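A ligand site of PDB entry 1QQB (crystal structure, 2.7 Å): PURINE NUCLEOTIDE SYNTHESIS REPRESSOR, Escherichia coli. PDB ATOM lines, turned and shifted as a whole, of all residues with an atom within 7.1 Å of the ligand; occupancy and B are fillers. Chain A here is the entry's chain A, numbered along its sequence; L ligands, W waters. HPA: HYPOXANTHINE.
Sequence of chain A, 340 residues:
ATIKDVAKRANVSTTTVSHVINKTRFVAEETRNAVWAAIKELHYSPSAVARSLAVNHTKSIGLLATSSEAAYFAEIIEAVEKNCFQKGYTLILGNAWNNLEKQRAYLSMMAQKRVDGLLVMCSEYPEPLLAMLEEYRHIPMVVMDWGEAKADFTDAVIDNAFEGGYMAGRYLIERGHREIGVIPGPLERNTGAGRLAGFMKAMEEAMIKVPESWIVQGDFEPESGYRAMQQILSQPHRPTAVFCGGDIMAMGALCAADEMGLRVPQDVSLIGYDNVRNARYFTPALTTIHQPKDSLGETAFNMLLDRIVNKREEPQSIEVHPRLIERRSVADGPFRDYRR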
ATOM      1  N   THR A  66       3.179   5.369 -12.190  1.00  0.00           N
ATOM      2  CA  THR A  66       3.247   4.754 -13.505  1.00  0.00           C
ATOM      3  C   THR A  66       4.655   4.934 -14.051  1.00  0.00           C
ATOM      4  O   THR A  66       5.366   3.957 -14.308  1.00  0.00           O
ATOM      5  CB  THR A  66       2.273   5.447 -14.426  1.00  0.00           C
ATOM      6  OG1 THR A  66       0.931   5.246 -13.956  1.00  0.00           O
ATOM      7  CG2 THR A  66       2.376   4.851 -15.753  1.00  0.00           C
ATOM      8  N   ALA A  70       7.922  11.892 -17.156  1.00  0.00           N
ATOM      9  CA  ALA A  70       6.930  12.736 -17.783  1.00  0.00           C
ATOM     10  C   ALA A  70       6.532  13.909 -16.925  1.00  0.00           C
ATOM     11  O   ALA A  70       6.127  13.760 -15.746  1.00  0.00           O
ATOM     12  CB  ALA A  70       5.697  11.935 -18.163  1.00  0.00           C
ATOM     13  N   ALA A  71       6.662  15.069 -17.551  1.00  0.00           N
ATOM     14  CA  ALA A  71       6.365  16.340 -16.969  1.00  0.00           C
ATOM     15  C   ALA A  71       5.160  16.309 -16.066  1.00  0.00           C
ATOM     16  O   ALA A  71       5.226  16.708 -14.912  1.00  0.00           O
ATOM     17  CB  ALA A  71       6.091  17.296 -18.053  1.00  0.00           C
ATOM     18  N   TYR A  72       4.063  15.852 -16.643  1.00  0.00           N
ATOM     19  CA  TYR A  72       2.831  15.809 -15.928  1.00  0.00           C
ATOM     20  C   TYR A  72       3.006  15.085 -14.589  1.00  0.00           C
ATOM     21  O   TYR A  72       2.729  15.641 -13.510  1.00  0.00           O
ATOM     22  CB  TYR A  72       1.817  15.157 -16.842  1.00  0.00           C
ATOM     23  CG  TYR A  72       0.467  14.959 -16.238  1.00  0.00           C
ATOM     24  CD1 TYR A  72      -0.390  16.017 -16.065  1.00  0.00           C
ATOM     25  CD2 TYR A  72       0.031  13.716 -15.872  1.00  0.00           C
ATOM     26  CE1 TYR A  72      -1.643  15.864 -15.519  1.00  0.00           C
ATOM     27  CE2 TYR A  72      -1.234  13.521 -15.342  1.00  0.00           C
ATOM     28  CZ  TYR A  72      -2.058  14.611 -15.149  1.00  0.00           C
ATOM     29  OH  TYR A  72      -3.296  14.441 -14.602  1.00  0.00           O
ATOM     30  N   PHE A  73       3.505  13.857 -14.669  1.00  0.00           N
ATOM     31  CA  PHE A  73       3.698  13.067 -13.484  1.00  0.00           C
ATOM     32  C   PHE A  73       4.671  13.687 -12.577  1.00  0.00           C
ATOM     33  O   PHE A  73       4.439  13.850 -11.378  1.00  0.00           O
ATOM     34  CB  PHE A  73       4.256  11.691 -13.834  1.00  0.00           C
ATOM     35  CG  PHE A  73       3.253  10.842 -14.555  1.00  0.00           C
ATOM     36  CD1 PHE A  73       1.922  11.057 -14.362  1.00  0.00           C
ATOM     37  CD2 PHE A  73       3.639   9.870 -15.434  1.00  0.00           C
ATOM     38  CE1 PHE A  73       1.020  10.297 -15.015  1.00  0.00           C
ATOM     39  CE2 PHE A  73       2.717   9.103 -16.116  1.00  0.00           C
ATOM     40  CZ  PHE A  73       1.429   9.314 -15.939  1.00  0.00           C
ATOM     41  N   SER A 123      -2.718   5.031 -14.035  1.00  0.00           N
ATOM     42  CA  SER A 123      -3.151   5.333 -15.405  1.00  0.00           C
ATOM     43  C   SER A 123      -4.238   4.455 -15.937  1.00  0.00           C
ATOM     44  O   SER A 123      -5.341   4.905 -16.125  1.00  0.00           O
ATOM     45  CB  SER A 123      -1.979   5.314 -16.375  1.00  0.00           C
ATOM     46  OG  SER A 123      -1.071   6.355 -16.052  1.00  0.00           O
ATOM     47  N   ASP A 145      -6.110   9.210 -10.205  1.00  0.00           N
ATOM     48  CA  ASP A 145      -6.326   9.455 -11.621  1.00  0.00           C
ATOM     49  C   ASP A 145      -7.547   8.923 -12.327  1.00  0.00           C
ATOM     50  O   ASP A 145      -7.535   8.667 -13.533  1.00  0.00           O
ATOM     51  CB  ASP A 145      -5.065   9.128 -12.404  1.00  0.00           C
ATOM     52  CG  ASP A 145      -4.534   7.696 -12.164  1.00  0.00           C
ATOM     53  OD1 ASP A 145      -5.313   6.842 -11.635  1.00  0.00           O
ATOM     54  OD2 ASP A 145      -3.368   7.420 -12.561  1.00  0.00           O
ATOM     55  N   ASP A 159     -10.743  14.826 -11.396  1.00  0.00           N
ATOM     56  CA  ASP A 159     -10.324  16.011 -12.173  1.00  0.00           C
ATOM     57  C   ASP A 159     -11.246  16.663 -13.219  1.00  0.00           C
ATOM     58  O   ASP A 159     -10.864  17.642 -13.807  1.00  0.00           O
ATOM     59  CB  ASP A 159      -8.987  15.715 -12.829  1.00  0.00           C
ATOM     60  CG  ASP A 159      -9.109  14.734 -13.972  1.00  0.00           C
ATOM     61  OD1 ASP A 159     -10.242  14.260 -14.234  1.00  0.00           O
ATOM     62  OD2 ASP A 159      -8.081  14.397 -14.621  1.00  0.00           O
ATOM     63  N   PRO A 186      -4.234   7.845 -24.717  1.00  0.00           N
ATOM     64  CA  PRO A 186      -4.834   6.504 -24.627  1.00  0.00           C
ATOM     65  C   PRO A 186      -6.260   6.515 -24.074  1.00  0.00           C
ATOM     66  O   PRO A 186      -6.551   7.075 -23.003  1.00  0.00           O
ATOM     67  CB  PRO A 186      -3.906   5.757 -23.693  1.00  0.00           C
ATOM     68  CG  PRO A 186      -2.673   6.574 -23.591  1.00  0.00           C
ATOM     69  CD  PRO A 186      -2.895   7.929 -24.158  1.00  0.00           C
ATOM     70  N   ARG A 189      -7.350   5.525 -20.495  1.00  0.00           N
ATOM     71  CA  ARG A 189      -7.087   6.410 -19.386  1.00  0.00           C
ATOM     72  C   ARG A 189      -8.137   7.483 -19.316  1.00  0.00           C
ATOM     73  O   ARG A 189      -8.810   7.770 -20.278  1.00  0.00           O
ATOM     74  CB  ARG A 189      -5.745   7.075 -19.582  1.00  0.00           C
ATOM     75  CG  ARG A 189      -4.715   6.166 -19.096  1.00  0.00           C
ATOM     76  CD  ARG A 189      -3.757   5.947 -20.144  1.00  0.00           C
ATOM     77  NE  ARG A 189      -2.639   6.786 -19.831  1.00  0.00           N
ATOM     78  CZ  ARG A 189      -1.406   6.311 -19.772  1.00  0.00           C
ATOM     79  NH1 ARG A 189      -1.223   5.032 -19.995  1.00  0.00           N
ATOM     80  NH2 ARG A 189      -0.377   7.092 -19.495  1.00  0.00           N
ATOM     81  N   ASN A 190      -8.246   8.074 -18.148  1.00  0.00           N
ATOM     82  CA  ASN A 190      -9.203   9.140 -17.894  1.00  0.00           C
ATOM     83  C   ASN A 190      -8.827  10.344 -18.728  1.00  0.00           C
ATOM     84  O   ASN A 190      -9.595  10.791 -19.556  1.00  0.00           O
ATOM     85  CB  ASN A 190      -9.159   9.517 -16.417  1.00  0.00           C
ATOM     86  CG  ASN A 190     -10.002  10.689 -16.145  1.00  0.00           C
ATOM     87  OD1 ASN A 190     -11.099  10.816 -16.716  1.00  0.00           O
ATOM     88  ND2 ASN A 190      -9.492  11.609 -15.334  1.00  0.00           N
ATOM     89  N   THR A 191      -7.610  10.840 -18.467  1.00  0.00           N
ATOM     90  CA  THR A 191      -7.032  11.979 -19.160  1.00  0.00           C
ATOM     91  C   THR A 191      -7.080  11.768 -20.694  1.00  0.00           C
ATOM     92  O   THR A 191      -6.952  12.745 -21.454  1.00  0.00           O
ATOM     93  CB  THR A 191      -5.582  12.228 -18.723  1.00  0.00           C
ATOM     94  OG1 THR A 191      -4.850  11.012 -18.889  1.00  0.00           O
ATOM     95  CG2 THR A 191      -5.464  12.674 -17.228  1.00  0.00           C
ATOM     96  N   GLY A 192      -7.279  10.506 -21.132  1.00  0.00           N
ATOM     97  CA  GLY A 192      -7.390  10.167 -22.557  1.00  0.00           C
ATOM     98  C   GLY A 192      -8.886  10.205 -22.968  1.00  0.00           C
ATOM     99  O   GLY A 192      -9.393  11.131 -23.582  1.00  0.00           O
ATOM    100  N   ARG A 195     -11.001  13.420 -21.766  1.00  0.00           N
ATOM    101  CA  ARG A 195     -10.772  14.702 -22.350  1.00  0.00           C
ATOM    102  C   ARG A 195     -11.431  14.765 -23.739  1.00  0.00           C
ATOM    103  O   ARG A 195     -12.077  15.747 -24.106  1.00  0.00           O
ATOM    104  CB  ARG A 195      -9.281  15.000 -22.340  1.00  0.00           C
ATOM    105  CG  ARG A 195      -8.733  15.371 -20.922  1.00  0.00           C
ATOM    106  CD  ARG A 195      -7.166  15.461 -20.885  1.00  0.00           C
ATOM    107  NE  ARG A 195      -6.547  15.591 -19.559  1.00  0.00           N
ATOM    108  CZ  ARG A 195      -5.258  15.829 -19.364  1.00  0.00           C
ATOM    109  NH1 ARG A 195      -4.437  16.001 -20.398  1.00  0.00           N
ATOM    110  NH2 ARG A 195      -4.791  15.895 -18.134  1.00  0.00           N
ATOM    111  N   ASP A 219       0.129   8.906 -27.324  1.00  0.00           N
ATOM    112  CA  ASP A 219       0.378   8.120 -26.114  1.00  0.00           C
ATOM    113  C   ASP A 219       0.936   9.054 -25.078  1.00  0.00           C
ATOM    114  O   ASP A 219       1.570   8.602 -24.141  1.00  0.00           O
ATOM    115  CB  ASP A 219       1.402   7.016 -26.420  1.00  0.00           C
ATOM    116  CG  ASP A 219       2.745   7.553 -26.869  1.00  0.00           C
ATOM    117  OD1 ASP A 219       2.997   8.778 -26.843  1.00  0.00           O
ATOM    118  OD2 ASP A 219       3.602   6.744 -27.237  1.00  0.00           O
ATOM    119  N   PHE A 220       0.710  10.349 -25.264  1.00  0.00           N
ATOM    120  CA  PHE A 220       1.210  11.426 -24.384  1.00  0.00           C
ATOM    121  C   PHE A 220       2.687  11.614 -24.554  1.00  0.00           C
ATOM    122  O   PHE A 220       3.304  12.274 -23.764  1.00  0.00           O
ATOM    123  CB  PHE A 220       1.009  11.164 -22.916  1.00  0.00           C
ATOM    124  CG  PHE A 220      -0.402  11.299 -22.484  1.00  0.00           C
ATOM    125  CD1 PHE A 220      -1.021  12.528 -22.506  1.00  0.00           C
ATOM    126  CD2 PHE A 220      -1.114  10.163 -22.049  1.00  0.00           C
ATOM    127  CE1 PHE A 220      -2.327  12.658 -22.095  1.00  0.00           C
ATOM    128  CE2 PHE A 220      -2.411  10.269 -21.665  1.00  0.00           C
ATOM    129  CZ  PHE A 220      -3.026  11.539 -21.684  1.00  0.00           C
ATOM    130  N   GLU A 221       3.270  11.032 -25.578  1.00  0.00           N
ATOM    131  CA  GLU A 221       4.703  11.230 -25.716  1.00  0.00           C
ATOM    132  C   GLU A 221       4.952  12.098 -26.938  1.00  0.00           C
ATOM    133  O   GLU A 221       4.274  11.984 -27.963  1.00  0.00           O
ATOM    134  CB  GLU A 221       5.456   9.897 -25.756  1.00  0.00           C
ATOM    135  CG  GLU A 221       5.435   9.138 -24.433  1.00  0.00           C
ATOM    136  CD  GLU A 221       6.557   9.520 -23.475  1.00  0.00           C
ATOM    137  OE1 GLU A 221       6.365  10.433 -22.630  1.00  0.00           O
ATOM    138  OE2 GLU A 221       7.617   8.848 -23.518  1.00  0.00           O
ATOM    139  N   GLY A 245      -4.408  16.503 -26.896  1.00  0.00           N
ATOM    140  CA  GLY A 245      -4.640  15.951 -25.572  1.00  0.00           C
ATOM    141  C   GLY A 245      -3.689  16.103 -24.388  1.00  0.00           C
ATOM    142  O   GLY A 245      -4.077  15.797 -23.266  1.00  0.00           O
ATOM    143  N   GLY A 246      -2.449  16.570 -24.627  1.00  0.00           N
ATOM    144  CA  GLY A 246      -1.436  16.774 -23.579  1.00  0.00           C
ATOM    145  C   GLY A 246      -0.308  17.702 -24.085  1.00  0.00           C
ATOM    146  O   GLY A 246       0.162  17.601 -25.228  1.00  0.00           O
ATOM    147  N   ASP A 247       0.138  18.613 -23.229  1.00  0.00           N
ATOM    148  CA  ASP A 247       1.189  19.539 -23.649  1.00  0.00           C
ATOM    149  C   ASP A 247       2.439  18.920 -24.301  1.00  0.00           C
ATOM    150  O   ASP A 247       2.986  19.406 -25.296  1.00  0.00           O
ATOM    151  CB  ASP A 247       1.527  20.474 -22.520  1.00  0.00           C
ATOM    152  CG  ASP A 247       0.334  21.323 -22.053  1.00  0.00           C
ATOM    153  OD1 ASP A 247      -0.745  21.271 -22.673  1.00  0.00           O
ATOM    154  OD2 ASP A 247       0.497  22.111 -21.077  1.00  0.00           O
ATOM    155  N   ILE A 248       2.907  17.823 -23.728  1.00  0.00           N
ATOM    156  CA  ILE A 248       4.107  17.215 -24.262  1.00  0.00           C
ATOM    157  C   ILE A 248       3.903  16.657 -25.661  1.00  0.00           C
ATOM    158  O   ILE A 248       4.737  16.851 -26.549  1.00  0.00           O
ATOM    159  CB  ILE A 248       4.733  16.185 -23.301  1.00  0.00           C
ATOM    160  CG1 ILE A 248       4.954  16.813 -21.941  1.00  0.00           C
ATOM    161  CG2 ILE A 248       6.089  15.679 -23.834  1.00  0.00           C
ATOM    162  CD1 ILE A 248       6.156  17.672 -21.930  1.00  0.00           C
ATOM    163  N   TYR A 273      -3.276  20.626 -23.406  1.00  0.00           N
ATOM    164  CA  TYR A 273      -3.928  20.237 -22.185  1.00  0.00           C
ATOM    165  C   TYR A 273      -2.944  19.720 -21.208  1.00  0.00           C
ATOM    166  O   TYR A 273      -2.226  18.749 -21.510  1.00  0.00           O
ATOM    167  CB  TYR A 273      -4.903  19.136 -22.450  1.00  0.00           C
ATOM    168  CG  TYR A 273      -5.966  19.095 -21.392  1.00  0.00           C
ATOM    169  CD1 TYR A 273      -5.631  19.127 -20.060  1.00  0.00           C
ATOM    170  CD2 TYR A 273      -7.293  19.041 -21.739  1.00  0.00           C
ATOM    171  CE1 TYR A 273      -6.609  19.082 -19.091  1.00  0.00           C
ATOM    172  CE2 TYR A 273      -8.285  18.989 -20.786  1.00  0.00           C
ATOM    173  CZ  TYR A 273      -7.942  19.016 -19.458  1.00  0.00           C
ATOM    174  OH  TYR A 273      -8.934  18.971 -18.489  1.00  0.00           O
ATOM    175  N   ASP A 274      -2.945  20.399 -20.058  1.00  0.00           N
ATOM    176  CA  ASP A 274      -2.109  20.121 -18.879  1.00  0.00           C
ATOM    177  C   ASP A 274      -1.561  21.341 -18.206  1.00  0.00           C
ATOM    178  O   ASP A 274      -1.580  21.482 -16.981  1.00  0.00           O
ATOM    179  CB  ASP A 274      -0.960  19.158 -19.192  1.00  0.00           C
ATOM    180  CG  ASP A 274      -1.396  17.692 -19.156  1.00  0.00           C
ATOM    181  OD1 ASP A 274      -2.598  17.411 -18.949  1.00  0.00           O
ATOM    182  OD2 ASP A 274      -0.584  16.802 -19.419  1.00  0.00           O
ATOM    183  N   VAL A 276       1.592  22.283 -18.369  1.00  0.00           N
ATOM    184  CA  VAL A 276       2.803  21.782 -17.751  1.00  0.00           C
ATOM    185  C   VAL A 276       3.745  22.956 -17.496  1.00  0.00           C
ATOM    186  O   VAL A 276       3.754  23.909 -18.244  1.00  0.00           O
ATOM    187  CB  VAL A 276       3.390  20.790 -18.735  1.00  0.00           C
ATOM    188  CG1 VAL A 276       4.743  21.269 -19.212  1.00  0.00           C
ATOM    189  CG2 VAL A 276       3.290  19.357 -18.208  1.00  0.00           C
ATOM    190  N   GLN A 291      -4.294  21.916 -15.652  1.00  0.00           N
ATOM    191  CA  GLN A 291      -4.763  20.953 -14.665  1.00  0.00           C
ATOM    192  C   GLN A 291      -4.102  21.344 -13.394  1.00  0.00           C
ATOM    193  O   GLN A 291      -2.888  21.528 -13.365  1.00  0.00           O
ATOM    194  CB  GLN A 291      -4.281  19.551 -14.969  1.00  0.00           C
ATOM    195  CG  GLN A 291      -4.552  18.592 -13.842  1.00  0.00           C
ATOM    196  CD  GLN A 291      -5.701  17.676 -14.158  1.00  0.00           C
ATOM    197  OE1 GLN A 291      -5.543  16.458 -14.182  1.00  0.00           O
ATOM    198  NE2 GLN A 291      -6.876  18.259 -14.411  1.00  0.00           N
HETATM  199  N1  HPA L   1       0.833  10.645 -19.154  1.00  0.00           N
HETATM  200  C2  HPA L   1       1.565  11.788 -19.381  1.00  0.00           C
HETATM  201  N3  HPA L   1       1.080  13.022 -19.333  1.00  0.00           N
HETATM  202  C4  HPA L   1      -0.251  12.995 -19.061  1.00  0.00           C
HETATM  203  C5  HPA L   1      -1.065  11.912 -18.790  1.00  0.00           C
HETATM  204  C6  HPA L   1      -0.512  10.608 -18.815  1.00  0.00           C
HETATM  205  O6  HPA L   1      -1.049   9.512 -18.589  1.00  0.00           O
HETATM  206  N7  HPA L   1      -2.359  12.333 -18.533  1.00  0.00           N
HETATM  207  C8  HPA L   1      -2.316  13.635 -18.653  1.00  0.00           C
HETATM  208  N9  HPA L   1      -1.061  14.101 -18.942  1.00  0.00           N
HETATM  209  O   HOH W   1       3.483  14.907 -19.573  1.00  0.00           O
HETATM  210  O   HOH W   2      -3.577  10.456 -16.084  1.00  0.00           O
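An oxygen (O6) of the ligand is in hydrogen-bond range of the guanidinium group (NH2) of Arg 189 (2.7 Å). A nitrogen (N9) of the ligand sits at hydrogen-bond distance from the side-chain carboxylate (OD2) of Asp 274 (2.8 Å). The side-chain hydroxyl of Thr 191 is in hydrogen-bond range of a nitrogen (N7) of the ligand.
OD1 of Asp 274 lies within salt-bridge range of NH1 of Arg 195, 2.7 Å away. O of Asp 274 lies within hydrogen-bond range of N of Gln 291 (3.1 Å). O of Thr 191 lies close to NE of Arg 195, 3.4 Å away. The side-chain hydroxyl (OH) of Tyr 72 sits at hydrogen-bond distance from the side-chain amide oxygen (OE1) of Gln 291 (3.0 Å). The guanidinium group (NH1) of Arg 195 is in hydrogen-bond range of the backbone carbonyl oxygen (O) of Gly 245.
Tyr 72 touches the ligand. Phe 73 touches the ligand (CZ to N1, 3.5 Å). Arg 195 touches the ligand. CZ of Phe 220 touches N7 of the ligand, at 3.3 Å. Hydrophobic or aromatic side chains that line the ligand: Tyr 72, Phe 73 and Phe 220. Of the 25 residues printed, 7 come within 4 Å of the ligand.
Water W1 bridges a nitrogen (N3) of the ligand (3.1 Å) and the backbone NH of Tyr 72 (3.1 Å). Water W2 bridges OG1 of Thr 191 (3.1 Å) and N7 of the ligand (3.3 Å).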
